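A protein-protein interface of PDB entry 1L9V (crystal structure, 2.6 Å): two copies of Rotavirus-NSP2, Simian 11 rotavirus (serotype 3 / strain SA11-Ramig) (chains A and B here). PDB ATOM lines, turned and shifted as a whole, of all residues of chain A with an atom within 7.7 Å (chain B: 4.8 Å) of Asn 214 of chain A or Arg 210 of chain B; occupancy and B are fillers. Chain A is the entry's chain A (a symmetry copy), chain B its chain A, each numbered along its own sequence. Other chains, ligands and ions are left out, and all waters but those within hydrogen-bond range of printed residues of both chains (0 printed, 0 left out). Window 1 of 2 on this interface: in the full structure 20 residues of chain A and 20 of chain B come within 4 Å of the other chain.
O of Leu 209 of chain B sits at hydrogen-bond distance from N of Asn 214 of chain B, 3.3 Å away.
O of Leu 209 of chain A sits at hydrogen-bond distance from N of Asn 214 of chain A, 3.3 Å away.
NZ of Lys 215 of chain A sits close to OD1 of Asn 214 of chain A (3.5 Å).
The backbone carbonyl oxygen (O) of Trp 211 of chain B lies within hydrogen-bond range of the side-chain amide nitrogen (ND2) of Asn 214 of chain A (3.1 Å).
The side-chain amide nitrogen of Asn 214 of chain B sits at hydrogen-bond distance from the backbone carbonyl oxygen of Trp 211 of chain A (3.1 Å).
The side-chain amide oxygen (OD1) of Asn 214 of chain B lies close to the side-chain amide oxygen (OD1) of Asn 214 of chain A (3.4 Å).
Among the printed residues, no Asp or Glu carboxylate lies within 4 Å of a Lys or Arg side-chain nitrogen of the other chain.
Arg 210 of chain A touches Asn 214 of chain B, and with the chains exchanged Asn 214 of chain A touches Arg 210 of chain B.
Trp 211 of chain A touches Asn 214 of chain B, and with the chains exchanged Asn 214 of chain A touches Trp 211 of chain B.
Asn 214 of chain A touches its own counterpart, Asn 214 of chain B.
Of the 7 pairs that touch across the chains among the printed residues, 5 have their exchanged pair printed and touching as well.
Arg 210 of chain A touches Asn 214 of chain B.
Asn 214 of chain A touches Arg 210 of chain B (ND2 to O, 3.8 Å).
Trp 211 of chain B touches Lys 215 of chain A (CZ3 to CD, 3.5 Å).
CE of Lys 215 of chain A touches NE2 of Gln 212 of chain B, at 3.6 Å.
Of chain B, only Arg 210 (3.8 Å), Trp 211 (3.1 Å) and Asn 214 (3.4 Å) come within 4 Å of Asn 214 of chain A.
Of the printed residues of chain B, Trp 211 of chain A touches Asn 214.
Printed residues of chain B within 4 Å of Arg 210 of chain A: Asn 214.
Of the printed residues of chain A, Asn 214 of chain B touches Arg 210 (3.8 Å), Trp 211 (3.1 Å) and Asn 214 (3.4 Å).
Of the printed residues of chain B, Lys 215 of chain A touches Trp 211 (3.5 Å) and Gln 212 (3.6 Å).
Of the printed residues of chain A, Gln 212 of chain B touches Lys 215.
Gln 212 of chain A touches none of the printed residues of chain B.
The nearest printed residue of chain B that does not touch Asn 214 of chain A is Gln 212 of chain B (5.2 Å).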
ATOM      1  N   ALA A 207       0.338 -18.831 -18.318  1.00  0.00           N
ATOM      2  CA  ALA A 207      -0.958 -19.489 -18.342  1.00  0.00           C
ATOM      3  C   ALA A 207      -1.277 -20.148 -17.000  1.00  0.00           C
ATOM      4  O   ALA A 207      -2.397 -20.038 -16.484  1.00  0.00           O
ATOM      5  CB  ALA A 207      -0.994 -20.524 -19.459  1.00  0.00           C
ATOM      6  N   GLU A 208      -0.283 -20.837 -16.447  1.00  0.00           N
ATOM      7  CA  GLU A 208      -0.422 -21.521 -15.167  1.00  0.00           C
ATOM      8  C   GLU A 208      -0.777 -20.496 -14.084  1.00  0.00           C
ATOM      9  O   GLU A 208      -1.663 -20.736 -13.264  1.00  0.00           O
ATOM     10  CB  GLU A 208       0.888 -22.245 -14.823  1.00  0.00           C
ATOM     11  CG  GLU A 208       0.870 -23.039 -13.525  1.00  0.00           C
ATOM     12  CD  GLU A 208      -0.083 -24.215 -13.563  1.00  0.00           C
ATOM     13  OE1 GLU A 208      -0.016 -25.013 -14.525  1.00  0.00           O
ATOM     14  OE2 GLU A 208      -0.895 -24.352 -12.624  1.00  0.00           O
ATOM     15  N   LEU A 209      -0.096 -19.352 -14.090  1.00  0.00           N
ATOM     16  CA  LEU A 209      -0.370 -18.314 -13.107  1.00  0.00           C
ATOM     17  C   LEU A 209      -1.770 -17.726 -13.300  1.00  0.00           C
ATOM     18  O   LEU A 209      -2.489 -17.485 -12.326  1.00  0.00           O
ATOM     19  CB  LEU A 209       0.703 -17.227 -13.180  1.00  0.00           C
ATOM     20  CG  LEU A 209       2.095 -17.738 -12.769  1.00  0.00           C
ATOM     21  CD1 LEU A 209       3.169 -16.729 -13.150  1.00  0.00           C
ATOM     22  CD2 LEU A 209       2.122 -18.011 -11.274  1.00  0.00           C
ATOM     23  N   ARG A 210      -2.179 -17.514 -14.546  1.00  0.00           N
ATOM     24  CA  ARG A 210      -3.518 -16.985 -14.783  1.00  0.00           C
ATOM     25  C   ARG A 210      -4.652 -17.953 -14.398  1.00  0.00           C
ATOM     26  O   ARG A 210      -5.715 -17.515 -13.946  1.00  0.00           O
ATOM     27  CB  ARG A 210      -3.689 -16.571 -16.244  1.00  0.00           C
ATOM     28  CG  ARG A 210      -3.126 -15.201 -16.563  1.00  0.00           C
ATOM     29  CD  ARG A 210      -3.328 -14.854 -18.022  1.00  0.00           C
ATOM     30  NE  ARG A 210      -2.594 -13.653 -18.406  1.00  0.00           N
ATOM     31  CZ  ARG A 210      -2.533 -13.178 -19.647  1.00  0.00           C
ATOM     32  NH1 ARG A 210      -3.166 -13.800 -20.632  1.00  0.00           N
ATOM     33  NH2 ARG A 210      -1.833 -12.081 -19.907  1.00  0.00           N
ATOM     34  N   TRP A 211      -4.444 -19.258 -14.561  1.00  0.00           N
ATOM     35  CA  TRP A 211      -5.510 -20.205 -14.240  1.00  0.00           C
ATOM     36  C   TRP A 211      -5.490 -20.738 -12.812  1.00  0.00           C
ATOM     37  O   TRP A 211      -6.495 -20.707 -12.103  1.00  0.00           O
ATOM     38  CB  TRP A 211      -5.487 -21.382 -15.218  1.00  0.00           C
ATOM     39  CG  TRP A 211      -6.849 -21.911 -15.477  1.00  0.00           C
ATOM     40  CD1 TRP A 211      -7.863 -21.284 -16.159  1.00  0.00           C
ATOM     41  CD2 TRP A 211      -7.396 -23.131 -14.980  1.00  0.00           C
ATOM     42  NE1 TRP A 211      -9.013 -22.043 -16.109  1.00  0.00           N
ATOM     43  CE2 TRP A 211      -8.757 -23.180 -15.390  1.00  0.00           C
ATOM     44  CE3 TRP A 211      -6.875 -24.188 -14.223  1.00  0.00           C
ATOM     45  CZ2 TRP A 211      -9.599 -24.240 -15.065  1.00  0.00           C
ATOM     46  CZ3 TRP A 211      -7.712 -25.246 -13.897  1.00  0.00           C
ATOM     47  CH2 TRP A 211      -9.065 -25.264 -14.319  1.00  0.00           C
ATOM     48  N   GLN A 212      -4.338 -21.221 -12.381  1.00  0.00           N
ATOM     49  CA  GLN A 212      -4.216 -21.779 -11.049  1.00  0.00           C
ATOM     50  C   GLN A 212      -3.989 -20.761  -9.928  1.00  0.00           C
ATOM     51  O   GLN A 212      -4.188 -21.081  -8.749  1.00  0.00           O
ATOM     52  CB  GLN A 212      -3.087 -22.809 -11.037  1.00  0.00           C
ATOM     53  CG  GLN A 212      -3.149 -23.725  -9.850  1.00  0.00           C
ATOM     54  CD  GLN A 212      -4.485 -24.428  -9.769  1.00  0.00           C
ATOM     55  OE1 GLN A 212      -4.856 -25.170 -10.674  1.00  0.00           O
ATOM     56  NE2 GLN A 212      -5.225 -24.187  -8.692  1.00  0.00           N
ATOM     57  N   TYR A 213      -3.583 -19.545 -10.291  1.00  0.00           N
ATOM     58  CA  TYR A 213      -3.292 -18.498  -9.310  1.00  0.00           C
ATOM     59  C   TYR A 213      -3.921 -17.135  -9.617  1.00  0.00           C
ATOM     60  O   TYR A 213      -3.373 -16.098  -9.250  1.00  0.00           O
ATOM     61  CB  TYR A 213      -1.767 -18.348  -9.172  1.00  0.00           C
ATOM     62  CG  TYR A 213      -1.091 -19.661  -8.870  1.00  0.00           C
ATOM     63  CD1 TYR A 213      -0.543 -20.446  -9.892  1.00  0.00           C
ATOM     64  CD2 TYR A 213      -1.103 -20.184  -7.572  1.00  0.00           C
ATOM     65  CE1 TYR A 213      -0.030 -21.725  -9.625  1.00  0.00           C
ATOM     66  CE2 TYR A 213      -0.596 -21.451  -7.296  1.00  0.00           C
ATOM     67  CZ  TYR A 213      -0.065 -22.217  -8.320  1.00  0.00           C
ATOM     68  OH  TYR A 213       0.423 -23.470  -8.027  1.00  0.00           O
ATOM     69  N   ASN A 214      -5.078 -17.144 -10.266  1.00  0.00           N
ATOM     70  CA  ASN A 214      -5.755 -15.906 -10.634  1.00  0.00           C
ATOM     71  C   ASN A 214      -5.793 -14.832  -9.536  1.00  0.00           C
ATOM     72  O   ASN A 214      -5.735 -13.635  -9.838  1.00  0.00           O
ATOM     73  CB  ASN A 214      -7.179 -16.208 -11.130  1.00  0.00           C
ATOM     74  CG  ASN A 214      -8.202 -16.242 -10.008  1.00  0.00           C
ATOM     75  OD1 ASN A 214      -8.097 -17.038  -9.069  1.00  0.00           O
ATOM     76  ND2 ASN A 214      -9.205 -15.372 -10.102  1.00  0.00           N
ATOM     77  N   LYS A 215      -5.880 -15.241  -8.273  1.00  0.00           N
ATOM     78  CA  LYS A 215      -5.922 -14.272  -7.177  1.00  0.00           C
ATOM     79  C   LYS A 215      -4.542 -13.861  -6.642  1.00  0.00           C
ATOM     80  O   LYS A 215      -4.425 -13.401  -5.510  1.00  0.00           O
ATOM     81  CB  LYS A 215      -6.783 -14.813  -6.037  1.00  0.00           C
ATOM     82  CG  LYS A 215      -8.234 -15.030  -6.433  1.00  0.00           C
ATOM     83  CD  LYS A 215      -9.074 -15.505  -5.265  1.00  0.00           C
ATOM     84  CE  LYS A 215      -8.635 -16.882  -4.773  1.00  0.00           C
ATOM     85  NZ  LYS A 215      -8.869 -17.951  -5.795  1.00  0.00           N
ATOM     86  N   PHE A 216      -3.499 -14.018  -7.451  1.00  0.00           N
ATOM     87  CA  PHE A 216      -2.157 -13.645  -7.014  1.00  0.00           C
ATOM     88  C   PHE A 216      -1.458 -12.663  -7.941  1.00  0.00           C
ATOM     89  O   PHE A 216      -1.551 -12.763  -9.173  1.00  0.00           O
ATOM     90  CB  PHE A 216      -1.268 -14.888  -6.840  1.00  0.00           C
ATOM     91  CG  PHE A 216      -1.617 -15.717  -5.631  1.00  0.00           C
ATOM     92  CD1 PHE A 216      -2.834 -16.394  -5.559  1.00  0.00           C
ATOM     93  CD2 PHE A 216      -0.737 -15.804  -4.552  1.00  0.00           C
ATOM     94  CE1 PHE A 216      -3.173 -17.143  -4.432  1.00  0.00           C
ATOM     95  CE2 PHE A 216      -1.063 -16.549  -3.421  1.00  0.00           C
ATOM     96  CZ  PHE A 216      -2.291 -17.223  -3.360  1.00  0.00           C
ATOM     97  N   ALA A 217      -0.772 -11.699  -7.332  1.00  0.00           N
ATOM     98  CA  ALA A 217      -0.015 -10.702  -8.074  1.00  0.00           C
ATOM     99  C   ALA A 217       1.318 -11.348  -8.420  1.00  0.00           C
ATOM    100  O   ALA A 217       1.844 -12.147  -7.652  1.00  0.00           O
ATOM    101  CB  ALA A 217       0.209  -9.476  -7.215  1.00  0.00           C
ATOM    102  N   ILE A 228       5.001 -14.809  -6.049  1.00  0.00           N
ATOM    103  CA  ILE A 228       3.556 -14.898  -6.226  1.00  0.00           C
ATOM    104  C   ILE A 228       2.837 -14.607  -4.918  1.00  0.00           C
ATOM    105  O   ILE A 228       2.600 -15.493  -4.096  1.00  0.00           O
ATOM    106  CB  ILE A 228       3.180 -16.291  -6.756  1.00  0.00           C
ATOM    107  CG1 ILE A 228       4.095 -16.630  -7.928  1.00  0.00           C
ATOM    108  CG2 ILE A 228       1.737 -16.319  -7.204  1.00  0.00           C
ATOM    109  CD1 ILE A 228       4.184 -15.531  -8.980  1.00  0.00           C
ATOM    110  N   TYR A 231      -2.837 -10.284  -3.999  1.00  0.00           N
ATOM    111  CA  TYR A 231      -3.068  -8.850  -4.134  1.00  0.00           C
ATOM    112  C   TYR A 231      -3.316  -8.070  -2.852  1.00  0.00           C
ATOM    113  O   TYR A 231      -2.994  -6.887  -2.775  1.00  0.00           O
ATOM    114  CB  TYR A 231      -4.232  -8.596  -5.087  1.00  0.00           C
ATOM    115  CG  TYR A 231      -3.918  -8.954  -6.520  1.00  0.00           C
ATOM    116  CD1 TYR A 231      -4.353 -10.153  -7.073  1.00  0.00           C
ATOM    117  CD2 TYR A 231      -3.185  -8.088  -7.320  1.00  0.00           C
ATOM    118  CE1 TYR A 231      -4.070 -10.475  -8.385  1.00  0.00           C
ATOM    119  CE2 TYR A 231      -2.893  -8.406  -8.638  1.00  0.00           C
ATOM    120  CZ  TYR A 231      -3.340  -9.599  -9.160  1.00  0.00           C
ATOM    121  OH  TYR A 231      -3.059  -9.903 -10.465  1.00  0.00           O
ATOM    122  N   LYS A 308      -8.920 -23.413 -19.936  1.00  0.00           N
ATOM    123  CA  LYS A 308     -10.312 -23.712 -19.645  1.00  0.00           C
ATOM    124  C   LYS A 308     -10.804 -24.762 -20.640  1.00  0.00           C
ATOM    125  O   LYS A 308     -11.345 -25.806 -20.246  1.00  0.00           O
ATOM    126  CB  LYS A 308     -11.152 -22.439 -19.766  1.00  0.00           C
ATOM    127  CG  LYS A 308     -12.635 -22.631 -19.519  1.00  0.00           C
ATOM    128  CD  LYS A 308     -13.422 -21.361 -19.839  1.00  0.00           C
ATOM    129  CE  LYS A 308     -13.045 -20.190 -18.922  1.00  0.00           C
ATOM    130  NZ  LYS A 308     -13.940 -19.008 -19.128  1.00  0.00           N
ATOM    131  N   VAL B 206     -21.730 -11.990 -10.945  1.00  0.00           N
ATOM    132  CA  VAL B 206     -20.812 -12.408 -12.002  1.00  0.00           C
ATOM    133  C   VAL B 206     -19.374 -12.102 -11.598  1.00  0.00           C
ATOM    134  O   VAL B 206     -18.449 -12.808 -11.986  1.00  0.00           O
ATOM    135  CB  VAL B 206     -21.122 -11.705 -13.345  1.00  0.00           C
ATOM    136  CG1 VAL B 206     -19.978 -11.943 -14.340  1.00  0.00           C
ATOM    137  CG2 VAL B 206     -22.445 -12.230 -13.911  1.00  0.00           C
ATOM    138  N   ALA B 207     -19.187 -11.060 -10.801  1.00  0.00           N
ATOM    139  CA  ALA B 207     -17.850 -10.691 -10.369  1.00  0.00           C
ATOM    140  C   ALA B 207     -17.288 -11.696  -9.362  1.00  0.00           C
ATOM    141  O   ALA B 207     -16.124 -12.108  -9.451  1.00  0.00           O
ATOM    142  CB  ALA B 207     -17.867  -9.293  -9.764  1.00  0.00           C
ATOM    143  N   GLU B 208     -18.127 -12.079  -8.403  1.00  0.00           N
ATOM    144  CA  GLU B 208     -17.750 -13.034  -7.369  1.00  0.00           C
ATOM    145  C   GLU B 208     -17.351 -14.360  -8.029  1.00  0.00           C
ATOM    146  O   GLU B 208     -16.343 -14.961  -7.661  1.00  0.00           O
ATOM    147  CB  GLU B 208     -18.925 -13.240  -6.402  1.00  0.00           C
ATOM    148  CG  GLU B 208     -18.653 -14.187  -5.242  1.00  0.00           C
ATOM    149  CD  GLU B 208     -17.606 -13.664  -4.282  1.00  0.00           C
ATOM    150  OE1 GLU B 208     -17.725 -12.501  -3.835  1.00  0.00           O
ATOM    151  OE2 GLU B 208     -16.663 -14.419  -3.962  1.00  0.00           O
ATOM    152  N   LEU B 209     -18.134 -14.804  -9.010  1.00  0.00           N
ATOM    153  CA  LEU B 209     -17.830 -16.048  -9.702  1.00  0.00           C
ATOM    154  C   LEU B 209     -16.532 -15.929 -10.506  1.00  0.00           C
ATOM    155  O   LEU B 209     -15.714 -16.853 -10.516  1.00  0.00           O
ATOM    156  CB  LEU B 209     -19.002 -16.448 -10.599  1.00  0.00           C
ATOM    157  CG  LEU B 209     -20.269 -16.796  -9.798  1.00  0.00           C
ATOM    158  CD1 LEU B 209     -21.478 -16.881 -10.719  1.00  0.00           C
ATOM    159  CD2 LEU B 209     -20.066 -18.108  -9.057  1.00  0.00           C
ATOM    160  N   ARG B 210     -16.320 -14.794 -11.162  1.00  0.00           N
ATOM    161  CA  ARG B 210     -15.082 -14.620 -11.916  1.00  0.00           C
ATOM    162  C   ARG B 210     -13.818 -14.546 -11.040  1.00  0.00           C
ATOM    163  O   ARG B 210     -12.751 -15.015 -11.449  1.00  0.00           O
ATOM    164  CB  ARG B 210     -15.153 -13.374 -12.798  1.00  0.00           C
ATOM    165  CG  ARG B 210     -15.883 -13.591 -14.108  1.00  0.00           C
ATOM    166  CD  ARG B 210     -15.916 -12.321 -14.930  1.00  0.00           C
ATOM    167  NE  ARG B 210     -16.808 -12.436 -16.079  1.00  0.00           N
ATOM    168  CZ  ARG B 210     -17.083 -11.438 -16.916  1.00  0.00           C
ATOM    169  NH1 ARG B 210     -16.533 -10.245 -16.736  1.00  0.00           N
ATOM    170  NH2 ARG B 210     -17.915 -11.631 -17.932  1.00  0.00           N
ATOM    171  N   TRP B 211     -13.919 -13.975  -9.842  1.00  0.00           N
ATOM    172  CA  TRP B 211     -12.733 -13.854  -8.997  1.00  0.00           C
ATOM    173  C   TRP B 211     -12.507 -15.015  -8.033  1.00  0.00           C
ATOM    174  O   TRP B 211     -11.423 -15.593  -7.972  1.00  0.00           O
ATOM    175  CB  TRP B 211     -12.776 -12.544  -8.205  1.00  0.00           C
ATOM    176  CG  TRP B 211     -11.418 -11.993  -7.978  1.00  0.00           C
ATOM    177  CD1 TRP B 211     -10.571 -11.467  -8.924  1.00  0.00           C
ATOM    178  CD2 TRP B 211     -10.692 -11.995  -6.750  1.00  0.00           C
ATOM    179  NE1 TRP B 211      -9.357 -11.147  -8.353  1.00  0.00           N
ATOM    180  CE2 TRP B 211      -9.402 -11.464  -7.022  1.00  0.00           C
ATOM    181  CE3 TRP B 211     -11.001 -12.400  -5.445  1.00  0.00           C
ATOM    182  CZ2 TRP B 211      -8.425 -11.330  -6.039  1.00  0.00           C
ATOM    183  CZ3 TRP B 211     -10.030 -12.268  -4.462  1.00  0.00           C
ATOM    184  CH2 TRP B 211      -8.751 -11.737  -4.766  1.00  0.00           C
ATOM    185  N   GLN B 212     -13.538 -15.367  -7.286  1.00  0.00           N
ATOM    186  CA  GLN B 212     -13.423 -16.439  -6.317  1.00  0.00           C
ATOM    187  C   GLN B 212     -13.592 -17.854  -6.879  1.00  0.00           C
ATOM    188  O   GLN B 212     -13.204 -18.831  -6.227  1.00  0.00           O
ATOM    189  CB  GLN B 212     -14.435 -16.213  -5.195  1.00  0.00           C
ATOM    190  CG  GLN B 212     -14.123 -17.012  -3.962  1.00  0.00           C
ATOM    191  CD  GLN B 212     -12.728 -16.722  -3.460  1.00  0.00           C
ATOM    192  OE1 GLN B 212     -12.414 -15.589  -3.107  1.00  0.00           O
ATOM    193  NE2 GLN B 212     -11.875 -17.741  -3.440  1.00  0.00           N
ATOM    194  N   TYR B 213     -14.160 -17.961  -8.079  1.00  0.00           N
ATOM    195  CA  TYR B 213     -14.413 -19.261  -8.705  1.00  0.00           C
ATOM    196  C   TYR B 213     -13.967 -19.371 -10.166  1.00  0.00           C
ATOM    197  O   TYR B 213     -14.557 -20.116 -10.945  1.00  0.00           O
ATOM    198  CB  TYR B 213     -15.913 -19.587  -8.594  1.00  0.00           C
ATOM    199  CG  TYR B 213     -16.411 -19.495  -7.174  1.00  0.00           C
ATOM    200  CD1 TYR B 213     -17.015 -18.326  -6.693  1.00  0.00           C
ATOM    201  CD2 TYR B 213     -16.173 -20.534  -6.267  1.00  0.00           C
ATOM    202  CE1 TYR B 213     -17.361 -18.196  -5.339  1.00  0.00           C
ATOM    203  CE2 TYR B 213     -16.513 -20.415  -4.922  1.00  0.00           C
ATOM    204  CZ  TYR B 213     -17.102 -19.249  -4.462  1.00  0.00           C
ATOM    205  OH  TYR B 213     -17.422 -19.150  -3.127  1.00  0.00           O
ATOM    206  N   ASN B 214     -12.913 -18.648 -10.524  1.00  0.00           N
ATOM    207  CA  ASN B 214     -12.416 -18.655 -11.895  1.00  0.00           C
ATOM    208  C   ASN B 214     -12.332 -20.040 -12.553  1.00  0.00           C
ATOM    209  O   ASN B 214     -12.546 -20.165 -13.763  1.00  0.00           O
ATOM    210  CB  ASN B 214     -11.050 -17.951 -11.966  1.00  0.00           C
ATOM    211  CG  ASN B 214      -9.885 -18.892 -11.712  1.00  0.00           C
ATOM    212  OD1 ASN B 214      -9.784 -19.514 -10.650  1.00  0.00           O
ATOM    213  ND2 ASN B 214      -8.993 -18.999 -12.694  1.00  0.00           N
ATOM    214  N   LYS B 297     -18.222 -12.762 -24.117  1.00  0.00           N
ATOM    215  CA  LYS B 297     -17.167 -13.057 -23.152  1.00  0.00           C
ATOM    216  C   LYS B 297     -16.950 -11.784 -22.344  1.00  0.00           C
ATOM    217  O   LYS B 297     -16.280 -11.782 -21.310  1.00  0.00           O
ATOM    218  CB  LYS B 297     -15.883 -13.461 -23.896  1.00  0.00           C
ATOM    219  CG  LYS B 297     -14.709 -13.910 -23.023  1.00  0.00           C
ATOM    220  CD  LYS B 297     -13.790 -12.751 -22.646  1.00  0.00           C
ATOM    221  CE  LYS B 297     -12.531 -13.247 -21.947  1.00  0.00           C
ATOM    222  NZ  LYS B 297     -11.600 -12.135 -21.606  1.00  0.00           N
ATOM    223  N   PRO B 299     -19.668  -9.637 -21.140  1.00  0.00           N
ATOM    224  CA  PRO B 299     -20.980  -9.111 -20.745  1.00  0.00           C
ATOM    225  C   PRO B 299     -20.770  -7.869 -19.889  1.00  0.00           C
ATOM    226  O   PRO B 299     -21.363  -6.817 -20.133  1.00  0.00           O
ATOM    227  CB  PRO B 299     -21.592 -10.265 -19.951  1.00  0.00           C
ATOM    228  CG  PRO B 299     -20.964 -11.474 -20.571  1.00  0.00           C
ATOM    229  CD  PRO B 299     -19.523 -11.040 -20.716  1.00  0.00           C
ATOM    230  N   PHE B 300     -19.906  -8.011 -18.889  1.00  0.00           N
ATOM    231  CA  PHE B 300     -19.567  -6.922 -17.986  1.00  0.00           C
ATOM    232  C   PHE B 300     -18.048  -6.817 -17.959  1.00  0.00           C
ATOM    233  O   PHE B 300     -17.452  -6.681 -16.893  1.00  0.00           O
ATOM    234  CB  PHE B 300     -20.067  -7.203 -16.565  1.00  0.00           C
ATOM    235  CG  PHE B 300     -21.487  -7.694 -16.496  1.00  0.00           C
ATOM    236  CD1 PHE B 300     -21.802  -9.005 -16.845  1.00  0.00           C
ATOM    237  CD2 PHE B 300     -22.507  -6.852 -16.072  1.00  0.00           C
ATOM    238  CE1 PHE B 300     -23.110  -9.470 -16.771  1.00  0.00           C
ATOM    239  CE2 PHE B 300     -23.819  -7.308 -15.993  1.00  0.00           C
ATOM    240  CZ  PHE B 300     -24.120  -8.622 -16.344  1.00  0.00           C
ATOM    241  N   LYS B 301     -17.432  -6.896 -19.135  1.00  0.00           N
ATOM    242  CA  LYS B 301     -15.980  -6.820 -19.249  1.00  0.00           C
ATOM    243  C   LYS B 301     -15.422  -5.728 -18.341  1.00  0.00           C
ATOM    244  O   LYS B 301     -15.744  -4.551 -18.504  1.00  0.00           O
ATOM    245  CB  LYS B 301     -15.574  -6.545 -20.700  1.00  0.00           C
ATOM    246  CG  LYS B 301     -14.088  -6.739 -20.968  1.00  0.00           C
ATOM    247  CD  LYS B 301     -13.656  -8.158 -20.620  1.00  0.00           C
ATOM    248  CE  LYS B 301     -12.151  -8.337 -20.729  1.00  0.00           C
ATOM    249  NZ  LYS B 301     -11.728  -9.688 -20.265  1.00  0.00           N
ATOM    250  N   GLY B 302     -14.591  -6.129 -17.385  1.00  0.00           N
ATOM    251  CA  GLY B 302     -14.011  -5.172 -16.459  1.00  0.00           C
ATOM    252  C   GLY B 302     -14.217  -5.555 -15.003  1.00  0.00           C
ATOM    253  O   GLY B 302     -13.539  -5.028 -14.119  1.00  0.00           O
ATOM    254  N   LEU B 303     -15.152  -6.467 -14.749  1.00  0.00           N
ATOM    255  CA  LEU B 303     -15.432  -6.916 -13.389  1.00  0.00           C
ATOM    256  C   LEU B 303     -14.163  -7.401 -12.709  1.00  0.00           C
ATOM    257  O   LEU B 303     -13.877  -7.038 -11.569  1.00  0.00           O
ATOM    258  CB  LEU B 303     -16.443  -8.065 -13.391  1.00  0.00           C
ATOM    259  CG  LEU B 303     -17.901  -7.802 -13.765  1.00  0.00           C
ATOM    260  CD1 LEU B 303     -18.711  -9.045 -13.464  1.00  0.00           C
ATOM    261  CD2 LEU B 303     -18.442  -6.613 -12.971  1.00  0.00           C
